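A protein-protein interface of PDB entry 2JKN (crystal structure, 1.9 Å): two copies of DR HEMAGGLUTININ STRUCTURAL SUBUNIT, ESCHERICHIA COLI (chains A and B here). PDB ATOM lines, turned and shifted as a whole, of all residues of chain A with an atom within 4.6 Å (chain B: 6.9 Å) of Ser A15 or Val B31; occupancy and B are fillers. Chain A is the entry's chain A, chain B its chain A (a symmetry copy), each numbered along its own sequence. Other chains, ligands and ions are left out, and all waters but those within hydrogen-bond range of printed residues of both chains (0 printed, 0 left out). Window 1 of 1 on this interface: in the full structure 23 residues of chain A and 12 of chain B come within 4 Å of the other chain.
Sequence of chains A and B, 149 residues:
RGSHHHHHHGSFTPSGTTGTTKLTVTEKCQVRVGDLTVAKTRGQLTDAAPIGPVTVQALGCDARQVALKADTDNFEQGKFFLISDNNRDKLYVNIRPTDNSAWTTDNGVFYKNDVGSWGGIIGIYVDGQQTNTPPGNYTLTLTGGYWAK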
ATOM      1  N   THR A  13      -6.025  14.398  26.260  1.00  0.00           N
ATOM      2  CA  THR A  13      -5.599  13.300  27.132  1.00  0.00           C
ATOM      3  C   THR A  13      -4.457  13.854  28.020  1.00  0.00           C
ATOM      4  O   THR A  13      -3.377  14.178  27.505  1.00  0.00           O
ATOM      5  CB  THR A  13      -5.063  12.126  26.283  1.00  0.00           C
ATOM      6  OG1 THR A  13      -6.097  11.649  25.417  1.00  0.00           O
ATOM      7  CG2 THR A  13      -4.556  10.994  27.162  1.00  0.00           C
ATOM      8  N   PRO A  14      -4.684  13.955  29.334  1.00  0.00           N
ATOM      9  CA  PRO A  14      -3.620  14.409  30.246  1.00  0.00           C
ATOM     10  C   PRO A  14      -2.479  13.405  30.201  1.00  0.00           C
ATOM     11  O   PRO A  14      -2.686  12.188  30.335  1.00  0.00           O
ATOM     12  CB  PRO A  14      -4.294  14.385  31.629  1.00  0.00           C
ATOM     13  CG  PRO A  14      -5.762  14.431  31.347  1.00  0.00           C
ATOM     14  CD  PRO A  14      -5.952  13.716  30.045  1.00  0.00           C
ATOM     15  N   SER A  15      -1.278  13.905  29.950  1.00  0.00           N
ATOM     16  CA  SER A  15      -0.116  13.036  29.847  1.00  0.00           C
ATOM     17  C   SER A  15       1.139  13.878  29.889  1.00  0.00           C
ATOM     18  O   SER A  15       1.651  14.280  28.865  1.00  0.00           O
ATOM     19  CB  SER A  15      -0.149  12.201  28.554  1.00  0.00           C
ATOM     20  OG  SER A  15       0.958  11.306  28.536  1.00  0.00           O
ATOM     21  N   GLY A  16       1.589  14.197  31.095  1.00  0.00           N
ATOM     22  CA  GLY A  16       2.724  15.080  31.247  1.00  0.00           C
ATOM     23  C   GLY A  16       2.660  15.756  32.613  1.00  0.00           C
ATOM     24  O   GLY A  16       1.886  15.359  33.487  1.00  0.00           O
ATOM     25  N   THR A  17       3.484  16.778  32.791  1.00  0.00           N
ATOM     26  CA  THR A  17       3.544  17.462  34.067  1.00  0.00           C
ATOM     27  C   THR A  17       2.804  18.804  34.037  1.00  0.00           C
ATOM     28  O   THR A  17       2.239  19.205  33.017  1.00  0.00           O
ATOM     29  CB  THR A  17       4.980  17.599  34.551  1.00  0.00           C
ATOM     30  OG1 THR A  17       5.716  18.416  33.630  1.00  0.00           O
ATOM     31  CG2 THR A  17       5.653  16.183  34.684  1.00  0.00           C
ATOM     32  N   VAL A  56       8.092  23.943  27.628  1.00  0.00           N
ATOM     33  CA  VAL A  56       7.386  22.747  27.211  1.00  0.00           C
ATOM     34  C   VAL A  56       8.409  21.850  26.531  1.00  0.00           C
ATOM     35  O   VAL A  56       9.106  22.280  25.600  1.00  0.00           O
ATOM     36  CB  VAL A  56       6.217  23.105  26.201  1.00  0.00           C
ATOM     37  CG1 VAL A  56       5.495  21.823  25.711  1.00  0.00           C
ATOM     38  CG2 VAL A  56       5.203  24.103  26.816  1.00  0.00           C
ATOM     39  N   GLN A  57       8.495  20.602  26.982  1.00  0.00           N
ATOM     40  CA  GLN A  57       9.371  19.617  26.353  1.00  0.00           C
ATOM     41  C   GLN A  57       8.584  18.307  26.166  1.00  0.00           C
ATOM     42  O   GLN A  57       8.274  17.620  27.138  1.00  0.00           O
ATOM     43  CB  GLN A  57      10.615  19.362  27.223  1.00  0.00           C
ATOM     44  CG  GLN A  57      11.629  20.562  27.252  1.00  0.00           C
ATOM     45  CD  GLN A  57      12.432  20.719  25.964  1.00  0.00           C
ATOM     46  OE1 GLN A  57      12.264  19.951  25.022  1.00  0.00           O
ATOM     47  NE2 GLN A  57      13.361  21.684  25.949  1.00  0.00           N
ATOM     48  N   ALA A  58       8.254  17.972  24.918  1.00  0.00           N
ATOM     49  CA  ALA A  58       7.521  16.728  24.641  1.00  0.00           C
ATOM     50  C   ALA A  58       8.475  15.616  24.233  1.00  0.00           C
ATOM     51  O   ALA A  58       9.531  15.869  23.636  1.00  0.00           O
ATOM     52  CB  ALA A  58       6.451  16.958  23.529  1.00  0.00           C
ATOM     53  N   CYS A  61       6.034  11.869  21.209  1.00  0.00           N
ATOM     54  CA  CYS A  61       4.829  12.426  20.586  1.00  0.00           C
ATOM     55  C   CYS A  61       4.950  12.614  19.071  1.00  0.00           C
ATOM     56  O   CYS A  61       4.314  13.493  18.495  1.00  0.00           O
ATOM     57  CB  CYS A  61       4.445  13.765  21.256  1.00  0.00           C
ATOM     58  SG  CYS A  61       4.185  13.605  23.071  1.00  0.00           S
ATOM     59  N   VAL A  66       0.893  17.814  20.528  1.00  0.00           N
ATOM     60  CA  VAL A  66       1.181  18.292  21.877  1.00  0.00           C
ATOM     61  C   VAL A  66       0.105  19.289  22.308  1.00  0.00           C
ATOM     62  O   VAL A  66      -0.367  20.092  21.498  1.00  0.00           O
ATOM     63  CB  VAL A  66       2.606  18.914  21.911  1.00  0.00           C
ATOM     64  CG1 VAL A  66       2.812  19.784  23.170  1.00  0.00           C
ATOM     65  CG2 VAL A  66       3.633  17.808  21.815  1.00  0.00           C
ATOM     66  N   ALA A  67      -0.296  19.223  23.574  1.00  0.00           N
ATOM     67  CA  ALA A  67      -1.342  20.107  24.081  1.00  0.00           C
ATOM     68  C   ALA A  67      -1.096  20.528  25.550  1.00  0.00           C
ATOM     69  O   ALA A  67      -0.404  19.839  26.307  1.00  0.00           O
ATOM     70  CB  ALA A  67      -2.759  19.416  23.937  1.00  0.00           C
ATOM     71  N   GLY A 144       0.306  19.310  30.804  1.00  0.00           N
ATOM     72  CA  GLY A 144       0.717  18.773  29.505  1.00  0.00           C
ATOM     73  C   GLY A 144      -0.050  17.507  29.115  1.00  0.00           C
ATOM     74  O   GLY A 144      -0.418  16.694  29.964  1.00  0.00           O
ATOM     75  N   GLY A 145      -0.211  17.307  27.815  1.00  0.00           N
ATOM     76  CA  GLY A 145      -0.883  16.122  27.321  1.00  0.00           C
ATOM     77  C   GLY A 145      -0.947  16.212  25.818  1.00  0.00           C
ATOM     78  O   GLY A 145      -0.113  16.866  25.184  1.00  0.00           O
ATOM     79  N   TYR A 146      -1.923  15.541  25.231  1.00  0.00           N
ATOM     80  CA  TYR A 146      -2.057  15.580  23.780  1.00  0.00           C
ATOM     81  C   TYR A 146      -3.510  15.653  23.324  1.00  0.00           C
ATOM     82  O   TYR A 146      -4.415  15.293  24.069  1.00  0.00           O
ATOM     83  CB  TYR A 146      -1.306  14.438  23.120  1.00  0.00           C
ATOM     84  CG  TYR A 146      -1.760  13.056  23.529  1.00  0.00           C
ATOM     85  CD1 TYR A 146      -1.089  12.341  24.527  1.00  0.00           C
ATOM     86  CD2 TYR A 146      -2.814  12.431  22.866  1.00  0.00           C
ATOM     87  CE1 TYR A 146      -1.484  11.056  24.879  1.00  0.00           C
ATOM     88  CE2 TYR A 146      -3.206  11.138  23.195  1.00  0.00           C
ATOM     89  CZ  TYR A 146      -2.541  10.456  24.201  1.00  0.00           C
ATOM     90  OH  TYR A 146      -2.952   9.181  24.535  1.00  0.00           O
ATOM     91  N   THR B  24       5.127  11.784  38.752  1.00  0.00           N
ATOM     92  CA  THR B  24       4.046  11.990  37.797  1.00  0.00           C
ATOM     93  C   THR B  24       4.131  10.840  36.789  1.00  0.00           C
ATOM     94  O   THR B  24       5.211  10.530  36.276  1.00  0.00           O
ATOM     95  CB  THR B  24       4.091  13.382  37.114  1.00  0.00           C
ATOM     96  OG1 THR B  24       3.851  14.422  38.091  1.00  0.00           O
ATOM     97  CG2 THR B  24       3.011  13.458  35.977  1.00  0.00           C
ATOM     98  N   VAL B  25       3.028  10.123  36.626  1.00  0.00           N
ATOM     99  CA  VAL B  25       2.960   9.009  35.670  1.00  0.00           C
ATOM    100  C   VAL B  25       2.300   9.561  34.398  1.00  0.00           C
ATOM    101  O   VAL B  25       1.299  10.255  34.473  1.00  0.00           O
ATOM    102  CB  VAL B  25       2.131   7.824  36.236  1.00  0.00           C
ATOM    103  CG1 VAL B  25       1.956   6.730  35.179  1.00  0.00           C
ATOM    104  CG2 VAL B  25       2.782   7.239  37.515  1.00  0.00           C
ATOM    105  N   THR B  26       2.814   9.180  33.233  1.00  0.00           N
ATOM    106  CA  THR B  26       2.266   9.685  31.977  1.00  0.00           C
ATOM    107  C   THR B  26       2.087   8.524  31.026  1.00  0.00           C
ATOM    108  O   THR B  26       2.448   7.404  31.345  1.00  0.00           O
ATOM    109  CB  THR B  26       3.260  10.708  31.330  1.00  0.00           C
ATOM    110  OG1 THR B  26       4.350   9.989  30.737  1.00  0.00           O
ATOM    111  CG2 THR B  26       3.828  11.672  32.396  1.00  0.00           C
ATOM    112  N   GLU B  27       1.629   8.823  29.813  1.00  0.00           N
ATOM    113  CA  GLU B  27       1.608   7.845  28.742  1.00  0.00           C
ATOM    114  C   GLU B  27       2.946   7.991  28.007  1.00  0.00           C
ATOM    115  O   GLU B  27       3.791   8.823  28.391  1.00  0.00           O
ATOM    116  CB  GLU B  27       0.442   8.127  27.770  1.00  0.00           C
ATOM    117  CG  GLU B  27      -0.937   8.029  28.412  1.00  0.00           C
ATOM    118  CD  GLU B  27      -2.039   7.952  27.390  1.00  0.00           C
ATOM    119  OE1 GLU B  27      -1.737   8.102  26.179  1.00  0.00           O
ATOM    120  OE2 GLU B  27      -3.205   7.748  27.790  1.00  0.00           O
ATOM    121  N   LYS B  28       3.131   7.197  26.948  1.00  0.00           N
ATOM    122  CA  LYS B  28       4.348   7.256  26.133  1.00  0.00           C
ATOM    123  C   LYS B  28       4.586   8.663  25.568  1.00  0.00           C
ATOM    124  O   LYS B  28       5.731   9.143  25.545  1.00  0.00           O
ATOM    125  CB  LYS B  28       4.253   6.259  24.973  1.00  0.00           C
ATOM    126  CG  LYS B  28       5.575   5.629  24.596  1.00  0.00           C
ATOM    127  CD  LYS B  28       6.105   6.200  23.292  1.00  0.00           C
ATOM    128  CE  LYS B  28       4.967   6.490  22.321  1.00  0.00           C
ATOM    129  NZ  LYS B  28       5.408   7.332  21.189  1.00  0.00           N
ATOM    130  N   CYS B  29       3.520   9.302  25.088  1.00  0.00           N
ATOM    131  CA  CYS B  29       3.604  10.678  24.606  1.00  0.00           C
ATOM    132  C   CYS B  29       3.453  11.504  25.864  1.00  0.00           C
ATOM    133  O   CYS B  29       2.382  11.543  26.483  1.00  0.00           O
ATOM    134  CB  CYS B  29       2.501  11.024  23.596  1.00  0.00           C
ATOM    135  SG  CYS B  29       2.311  12.838  23.281  1.00  0.00           S
ATOM    136  N   GLN B  30       4.575  12.084  26.274  1.00  0.00           N
ATOM    137  CA  GLN B  30       4.736  12.724  27.563  1.00  0.00           C
ATOM    138  C   GLN B  30       5.122  14.186  27.373  1.00  0.00           C
ATOM    139  O   GLN B  30       6.120  14.481  26.735  1.00  0.00           O
ATOM    140  CB  GLN B  30       5.890  12.007  28.246  1.00  0.00           C
ATOM    141  CG  GLN B  30       6.320  12.546  29.586  1.00  0.00           C
ATOM    142  CD  GLN B  30       7.523  11.790  30.089  1.00  0.00           C
ATOM    143  OE1 GLN B  30       8.646  12.067  29.670  1.00  0.00           O
ATOM    144  NE2 GLN B  30       7.275  10.700  30.807  1.00  0.00           N
ATOM    145  N   VAL B  31       4.344  15.084  27.958  1.00  0.00           N
ATOM    146  CA  VAL B  31       4.572  16.535  27.783  1.00  0.00           C
ATOM    147  C   VAL B  31       4.977  17.214  29.099  1.00  0.00           C
ATOM    148  O   VAL B  31       4.157  17.433  29.981  1.00  0.00           O
ATOM    149  CB  VAL B  31       3.368  17.204  27.120  1.00  0.00           C
ATOM    150  CG1 VAL B  31       3.624  18.729  26.907  1.00  0.00           C
ATOM    151  CG2 VAL B  31       3.067  16.505  25.769  1.00  0.00           C
ATOM    152  N   ARG B  32       6.272  17.475  29.238  1.00  0.00           N
ATOM    153  CA  ARG B  32       6.798  18.089  30.444  1.00  0.00           C
ATOM    154  C   ARG B  32       6.634  19.601  30.396  1.00  0.00           C
ATOM    155  O   ARG B  32       7.200  20.267  29.528  1.00  0.00           O
ATOM    156  CB  ARG B  32       8.270  17.719  30.613  1.00  0.00           C
ATOM    157  CG  ARG B  32       8.469  16.243  30.905  1.00  0.00           C
ATOM    158  CD  ARG B  32       9.914  15.825  30.783  1.00  0.00           C
ATOM    159  NE  ARG B  32      10.046  14.377  30.952  1.00  0.00           N
ATOM    160  CZ  ARG B  32      10.486  13.782  32.062  1.00  0.00           C
ATOM    161  NH1 ARG B  32      10.862  14.508  33.115  1.00  0.00           N
ATOM    162  NH2 ARG B  32      10.568  12.459  32.111  1.00  0.00           N
ATOM    163  N   VAL B  33       5.890  20.127  31.357  1.00  0.00           N
ATOM    164  CA  VAL B  33       5.599  21.559  31.436  1.00  0.00           C
ATOM    165  C   VAL B  33       6.266  22.157  32.677  1.00  0.00           C
ATOM    166  O   VAL B  33       6.083  21.665  33.792  1.00  0.00           O
ATOM    167  CB  VAL B  33       4.046  21.812  31.468  1.00  0.00           C
ATOM    168  CG1 VAL B  33       3.742  23.318  31.387  1.00  0.00           C
ATOM    169  CG2 VAL B  33       3.349  21.066  30.305  1.00  0.00           C
ATOM    170  N   PRO B 135      -2.384   7.663  34.353  1.00  0.00           N
ATOM    171  CA  PRO B 135      -1.542   8.865  34.395  1.00  0.00           C
ATOM    172  C   PRO B 135      -2.098   9.811  35.468  1.00  0.00           C
ATOM    173  O   PRO B 135      -3.313   9.928  35.653  1.00  0.00           O
ATOM    174  CB  PRO B 135      -1.718   9.469  33.002  1.00  0.00           C
ATOM    175  CG  PRO B 135      -1.951   8.266  32.128  1.00  0.00           C
ATOM    176  CD  PRO B 135      -2.794   7.330  32.970  1.00  0.00           C
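The side-chain hydroxyl (OG) of Ser A15 lies within hydrogen-bond range of the backbone NH (N) of Glu B27 (2.9 Å).
OG of Ser A15 is in hydrogen-bond range of O of Cys B29 (2.5 Å).
The backbone carbonyl oxygen (O) of Ser A15 is in hydrogen-bond range of the backbone NH (N) of Val B31, at 3.0 Å.
N of Thr A17 is in hydrogen-bond range of O of Val B31.
The side-chain hydroxyl of Thr A17 is in hydrogen-bond range of the backbone NH of Val B33.
The backbone carbonyl oxygen (O) of Arg B32 lies within hydrogen-bond range of the backbone NH (N) of Gln A57, at 2.9 Å.
SG of Cys A61 forms a disulfide with SG of Cys B29, 2.0 Å away.
SG of Cys A61 lies within hydrogen-bond range of N of Gln B30 (3.6 Å).
OH of Tyr A146 lies close to OE1 of Glu B27.
The backbone NH (N) of Thr A13 sits at hydrogen-bond distance from the backbone carbonyl oxygen (O) of Tyr A146 (2.9 Å).
The backbone NH (N) of Ser A15 is in hydrogen-bond range of the backbone carbonyl oxygen (O) of Gly A144 (2.9 Å).
N of Gly A16 sits at hydrogen-bond distance from O of Gly A144, at 3.4 Å.
The backbone carbonyl oxygen (O) of Thr A17 is in hydrogen-bond range of the backbone NH (N) of Gly A144.
O of Gly A145 sits at hydrogen-bond distance from N of Ala A67 (2.9 Å).
OE1 of Gln B30 is in hydrogen-bond range of NE of Arg B32, 3.0 Å away.
Among the printed residues, pairs that only touch across the chains: Thr A13 with Glu B27, Pro A14 with Pro B135, Ser A15 with Thr B26, Ser A15 with Gln B30, Gly A16 with Thr B24, Gly A16 with Thr B26, Gly A16 with Val B31, Thr A17 with Arg B32, Val A56 with Val B31, Val A56 with Arg B32, Gln A57 with Gln B30, Gln A57 with Val B31, Ala A58 with Gln B30, Val A66 with Val B31, Gly A144 with Val B31, Gly A144 with Val B33, Gly A145 with Val B31 and Tyr A146 with Cys B29.
Of the printed residues of chain B, Ser A15 touches Thr B26 (3.7 Å), Glu B27 (2.9 Å), Cys B29 (2.5 Å), Gln B30 (3.7 Å) and Val B31 (3.0 Å).
Val B31 touches just these residues of chain A: Ser A15, Gly A16, Thr A17, Val A56, Gln A57, Val A66, Gly A144 and Gly A145.
Printed residues of chain B within 4 Å of Ala A58: Gln B30.
Of the printed residues of chain B, Val A66 touches Val B31.
Of the printed residues of chain B, Gly A144 touches Val B31 and Val B33.
Printed residues of chain A within 4 Å of Glu B27: Thr A13, Ser A15 and Tyr A146.
Of the printed residues of chain A, Val B33 touches Thr A17 (2.9 Å) and Gly A144 (3.5 Å).
The nearest printed residue of chain A that does not touch Glu B27 is Pro A14 (4.9 Å).
Printed residues of chain B that touch a printed residue of chain A: Thr B24, Thr B26, Glu B27, Cys B29, Gln B30, Val B31, Arg B32, Val B33 and Pro B135.
Hydrophobic or aromatic side chains of chain A that line the printed part of chain B: Val A56, Val A66 and Tyr A146.
Among the printed residues, no Asp or Glu carboxylate lies within 4 Å of a Lys or Arg side-chain nitrogen of the other chain.
No position is printed for both chains.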
